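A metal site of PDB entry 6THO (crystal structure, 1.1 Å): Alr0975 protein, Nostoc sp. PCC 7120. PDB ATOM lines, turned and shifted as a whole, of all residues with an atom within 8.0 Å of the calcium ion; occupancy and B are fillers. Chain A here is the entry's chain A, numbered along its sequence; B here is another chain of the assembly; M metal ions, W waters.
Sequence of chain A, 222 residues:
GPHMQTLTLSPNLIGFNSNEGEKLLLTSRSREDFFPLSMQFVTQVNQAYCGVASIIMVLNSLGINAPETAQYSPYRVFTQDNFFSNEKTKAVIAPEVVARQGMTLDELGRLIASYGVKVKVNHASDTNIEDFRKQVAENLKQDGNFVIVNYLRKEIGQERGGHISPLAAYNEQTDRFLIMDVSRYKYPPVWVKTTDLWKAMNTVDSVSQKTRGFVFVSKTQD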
ATOM      1  N   PHE A  16      21.615 -21.728 -24.449  1.00  0.00           N
ATOM      2  CA  PHE A  16      20.597 -22.707 -24.817  1.00  0.00           C
ATOM      3  C   PHE A  16      20.547 -23.869 -23.833  1.00  0.00           C
ATOM      4  O   PHE A  16      19.455 -24.380 -23.537  1.00  0.00           O
ATOM      5  CB  PHE A  16      20.931 -23.204 -26.230  1.00  0.00           C
ATOM      6  CG  PHE A  16      19.994 -24.255 -26.750  1.00  0.00           C
ATOM      7  CD1 PHE A  16      18.687 -23.936 -27.060  1.00  0.00           C
ATOM      8  CD2 PHE A  16      20.435 -25.551 -26.955  1.00  0.00           C
ATOM      9  CE1 PHE A  16      17.829 -24.897 -27.548  1.00  0.00           C
ATOM     10  CE2 PHE A  16      19.574 -26.519 -27.449  1.00  0.00           C
ATOM     11  CZ  PHE A  16      18.280 -26.185 -27.750  1.00  0.00           C
ATOM     12  N   ASN A  17      21.697 -24.299 -23.320  1.00  0.00           N
ATOM     13  CA  ASN A  17      21.773 -25.424 -22.394  1.00  0.00           C
ATOM     14  C   ASN A  17      21.597 -25.009 -20.935  1.00  0.00           C
ATOM     15  O   ASN A  17      22.029 -25.749 -20.037  1.00  0.00           O
ATOM     16  CB  ASN A  17      23.105 -26.158 -22.568  1.00  0.00           C
ATOM     17  CG  ASN A  17      24.300 -25.216 -22.534  1.00  0.00           C
ATOM     18  OD1 ASN A  17      24.164 -24.026 -22.831  1.00  0.00           O
ATOM     19  ND2 ASN A  17      25.469 -25.743 -22.204  1.00  0.00           N
ATOM     20  N   SER A  18      21.018 -23.850 -20.667  1.00  0.00           N
ATOM     21  CA  SER A  18      20.637 -23.462 -19.319  1.00  0.00           C
ATOM     22  C   SER A  18      19.174 -23.806 -19.089  1.00  0.00           C
ATOM     23  O   SER A  18      18.401 -23.981 -20.021  1.00  0.00           O
ATOM     24  CB  SER A  18      20.830 -21.955 -19.104  1.00  0.00           C
ATOM     25  OG  SER A  18      19.878 -21.213 -19.852  1.00  0.00           O
ATOM     26  N   ASN A  19      18.791 -23.892 -17.813  1.00  0.00           N
ATOM     27  CA  ASN A  19      17.377 -24.099 -17.535  1.00  0.00           C
ATOM     28  C   ASN A  19      16.514 -23.005 -18.163  1.00  0.00           C
ATOM     29  O   ASN A  19      15.482 -23.297 -18.784  1.00  0.00           O
ATOM     30  CB  ASN A  19      17.131 -24.156 -16.029  1.00  0.00           C
ATOM     31  CG  ASN A  19      17.633 -25.444 -15.413  1.00  0.00           C
ATOM     32  OD1 ASN A  19      17.827 -26.442 -16.107  1.00  0.00           O
ATOM     33  ND2 ASN A  19      17.835 -25.428 -14.102  1.00  0.00           N
ATOM     34  N   GLU A  20      16.938 -21.752 -18.035  1.00  0.00           N
ATOM     35  CA  GLU A  20      16.174 -20.673 -18.658  1.00  0.00           C
ATOM     36  C   GLU A  20      16.192 -20.794 -20.181  1.00  0.00           C
ATOM     37  O   GLU A  20      15.160 -20.596 -20.834  1.00  0.00           O
ATOM     38  CB  GLU A  20      16.731 -19.313 -18.233  1.00  0.00           C
ATOM     39  CG  GLU A  20      16.013 -18.110 -18.851  1.00  0.00           C
ATOM     40  CD  GLU A  20      14.674 -17.825 -18.182  1.00  0.00           C
ATOM     41  OE1 GLU A  20      13.923 -16.951 -18.679  1.00  0.00           O
ATOM     42  OE2 GLU A  20      14.371 -18.472 -17.161  1.00  0.00           O
ATOM     43  N   GLY A  21      17.353 -21.134 -20.761  1.00  0.00           N
ATOM     44  CA  GLY A  21      17.448 -21.243 -22.213  1.00  0.00           C
ATOM     45  C   GLY A  21      16.567 -22.347 -22.766  1.00  0.00           C
ATOM     46  O   GLY A  21      15.978 -22.197 -23.840  1.00  0.00           O
ATOM     47  N   GLU A  22      16.486 -23.467 -22.056  1.00  0.00           N
ATOM     48  CA  GLU A  22      15.550 -24.526 -22.450  1.00  0.00           C
ATOM     49  C   GLU A  22      14.117 -24.010 -22.431  1.00  0.00           C
ATOM     50  O   GLU A  22      13.361 -24.226 -23.384  1.00  0.00           O
ATOM     51  CB  GLU A  22      15.690 -25.725 -21.506  1.00  0.00           C
ATOM     52  CG  GLU A  22      17.063 -26.394 -21.510  1.00  0.00           C
ATOM     53  CD  GLU A  22      17.188 -27.467 -20.429  1.00  0.00           C
ATOM     54  OE1 GLU A  22      16.183 -27.762 -19.763  1.00  0.00           O
ATOM     55  OE2 GLU A  22      18.299 -28.011 -20.243  1.00  0.00           O
ATOM     56  N   LYS A  23      13.752 -23.301 -21.355  1.00  0.00           N
ATOM     57  CA  LYS A  23      12.402 -22.745 -21.238  1.00  0.00           C
ATOM     58  C   LYS A  23      12.085 -21.776 -22.380  1.00  0.00           C
ATOM     59  O   LYS A  23      10.968 -21.734 -22.874  1.00  0.00           O
ATOM     60  CB  LYS A  23      12.238 -22.045 -19.877  1.00  0.00           C
ATOM     61  CG  LYS A  23      10.997 -21.141 -19.744  1.00  0.00           C
ATOM     62  CD  LYS A  23      10.799 -20.586 -18.324  1.00  0.00           C
ATOM     63  CE  LYS A  23      11.979 -19.738 -17.874  1.00  0.00           C
ATOM     64  NZ  LYS A  23      11.681 -18.841 -16.718  1.00  0.00           N
ATOM     65  N   ARG B  31      13.458 -35.232 -21.290  1.00  0.00           N
ATOM     66  CA  ARG B  31      14.104 -34.669 -22.475  1.00  0.00           C
ATOM     67  C   ARG B  31      15.286 -33.771 -22.137  1.00  0.00           C
ATOM     68  O   ARG B  31      15.748 -33.043 -23.018  1.00  0.00           O
ATOM     69  CB  ARG B  31      13.073 -33.897 -23.294  1.00  0.00           C
ATOM     70  CG  ARG B  31      12.444 -32.750 -22.481  1.00  0.00           C
ATOM     71  CD  ARG B  31      11.400 -31.951 -23.237  1.00  0.00           C
ATOM     72  NE  ARG B  31      10.832 -30.936 -22.359  1.00  0.00           N
ATOM     73  CZ  ARG B  31       9.661 -30.338 -22.556  1.00  0.00           C
ATOM     74  NH1 ARG B  31       9.244 -29.433 -21.689  1.00  0.00           N
ATOM     75  NH2 ARG B  31       8.937 -30.629 -23.615  1.00  0.00           N
ATOM     76  N   GLU B  32      15.782 -33.807 -20.908  1.00  0.00           N
ATOM     77  CA  GLU B  32      16.896 -32.920 -20.555  1.00  0.00           C
ATOM     78  C   GLU B  32      18.105 -33.185 -21.450  1.00  0.00           C
ATOM     79  O   GLU B  32      18.780 -32.247 -21.899  1.00  0.00           O
ATOM     80  CB  GLU B  32      17.280 -33.099 -19.085  1.00  0.00           C
ATOM     81  CG  GLU B  32      16.260 -32.567 -18.108  1.00  0.00           C
ATOM     82  CD  GLU B  32      15.879 -31.152 -18.402  1.00  0.00           C
ATOM     83  OE1 GLU B  32      16.793 -30.292 -18.400  1.00  0.00           O
ATOM     84  OE2 GLU B  32      14.689 -30.910 -18.661  1.00  0.00           O
ATOM     85  N   ASP B  33      18.378 -34.456 -21.771  1.00  0.00           N
ATOM     86  CA  ASP B  33      19.583 -34.764 -22.529  1.00  0.00           C
ATOM     87  C   ASP B  33      19.518 -34.246 -23.955  1.00  0.00           C
ATOM     88  O   ASP B  33      20.565 -34.126 -24.594  1.00  0.00           O
ATOM     89  CB  ASP B  33      19.852 -36.277 -22.532  1.00  0.00           C
ATOM     90  CG  ASP B  33      20.236 -36.817 -21.167  1.00  0.00           C
ATOM     91  OD1 ASP B  33      20.444 -36.028 -20.222  1.00  0.00           O
ATOM     92  OD2 ASP B  33      20.361 -38.057 -21.037  1.00  0.00           O
ATOM     93  N   PHE B  35      19.003 -31.335 -25.051  1.00  0.00           N
ATOM     94  CA  PHE B  35      19.618 -30.025 -25.256  1.00  0.00           C
ATOM     95  C   PHE B  35      21.118 -30.139 -25.467  1.00  0.00           C
ATOM     96  O   PHE B  35      21.605 -29.714 -26.523  1.00  0.00           O
ATOM     97  CB  PHE B  35      19.167 -29.060 -24.163  1.00  0.00           C
ATOM     98  CG  PHE B  35      17.689 -28.795 -24.207  1.00  0.00           C
ATOM     99  CD1 PHE B  35      17.179 -27.797 -25.002  1.00  0.00           C
ATOM    100  CD2 PHE B  35      16.809 -29.578 -23.484  1.00  0.00           C
ATOM    101  CE1 PHE B  35      15.831 -27.545 -25.066  1.00  0.00           C
ATOM    102  CE2 PHE B  35      15.454 -29.333 -23.539  1.00  0.00           C
ATOM    103  CZ  PHE B  35      14.973 -28.334 -24.343  1.00  0.00           C
ATOM    104  N   PRO B  36      21.893 -30.737 -24.558  1.00  0.00           N
ATOM    105  CA  PRO B  36      23.331 -30.862 -24.831  1.00  0.00           C
ATOM    106  C   PRO B  36      23.642 -31.765 -26.013  1.00  0.00           C
ATOM    107  O   PRO B  36      24.598 -31.487 -26.767  1.00  0.00           O
ATOM    108  CB  PRO B  36      23.902 -31.432 -23.513  1.00  0.00           C
ATOM    109  CG  PRO B  36      22.689 -32.024 -22.802  1.00  0.00           C
ATOM    110  CD  PRO B  36      21.551 -31.119 -23.187  1.00  0.00           C
ATOM    111  N   LYS B 141      15.932 -37.521 -17.896  1.00  0.00           N
ATOM    112  CA  LYS B 141      15.543 -36.359 -17.118  1.00  0.00           C
ATOM    113  C   LYS B 141      16.716 -35.683 -16.408  1.00  0.00           C
ATOM    114  O   LYS B 141      16.560 -34.554 -15.922  1.00  0.00           O
ATOM    115  CB  LYS B 141      14.525 -36.763 -16.036  1.00  0.00           C
ATOM    116  CG  LYS B 141      13.163 -37.247 -16.515  1.00  0.00           C
ATOM    117  CD  LYS B 141      12.273 -37.578 -15.320  1.00  0.00           C
ATOM    118  CE  LYS B 141      10.854 -37.939 -15.723  1.00  0.00           C
ATOM    119  NZ  LYS B 141      10.797 -39.208 -16.464  1.00  0.00           N
ATOM    120  N   GLN B 142      17.866 -36.352 -16.323  1.00  0.00           N
ATOM    121  CA  GLN B 142      18.966 -35.943 -15.473  1.00  0.00           C
ATOM    122  C   GLN B 142      20.118 -35.362 -16.274  1.00  0.00           C
ATOM    123  O   GLN B 142      20.569 -35.981 -17.232  1.00  0.00           O
ATOM    124  CB  GLN B 142      19.536 -37.135 -14.694  1.00  0.00           C
ATOM    125  CG  GLN B 142      18.581 -37.711 -13.682  1.00  0.00           C
ATOM    126  CD  GLN B 142      19.048 -39.043 -13.113  1.00  0.00           C
ATOM    127  OE1 GLN B 142      19.817 -39.770 -13.741  1.00  0.00           O
ATOM    128  NE2 GLN B 142      18.555 -39.363 -11.930  1.00  0.00           N
ATOM    129  N   ASP B 143      20.620 -34.197 -15.865  1.00  0.00           N
ATOM    130  CA  ASP B 143      21.838 -33.648 -16.442  1.00  0.00           C
ATOM    131  C   ASP B 143      23.060 -34.385 -15.932  1.00  0.00           C
ATOM    132  O   ASP B 143      23.015 -35.065 -14.900  1.00  0.00           O
ATOM    133  CB  ASP B 143      21.990 -32.179 -16.072  1.00  0.00           C
ATOM    134  CG  ASP B 143      21.135 -31.282 -16.908  1.00  0.00           C
ATOM    135  OD1 ASP B 143      20.835 -31.659 -18.046  1.00  0.00           O
ATOM    136  OD2 ASP B 143      20.757 -30.189 -16.429  1.00  0.00           O
HETATM  137 CA    CA M   1      17.560 -28.225 -17.745  1.00  0.00          CA
HETATM  138  O   HOH W   1      18.431 -29.585 -15.841  1.00  0.00           O
HETATM  139  O   HOH W   2      15.378 -27.917 -16.909  1.00  0.00           O
HETATM  140  O   HOH W   3      19.893 -27.399 -17.929  1.00  0.00           O
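Asp 143 of chain B touches the calcium ion.
The backbone carbonyl oxygen (O) of Phe 16 lies within hydrogen-bond range of the backbone NH (N) of Glu 22 (3.4 Å).
The calcium ion is bound by OE1 of Glu 32 of chain B, water W2, OD1 of Asn 19, water W3, OE1 of Glu 22, water W1 and OE2 of Glu 22.
Water W3 bridges OD2 of Asp 143 of chain B and O of Asn 17.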
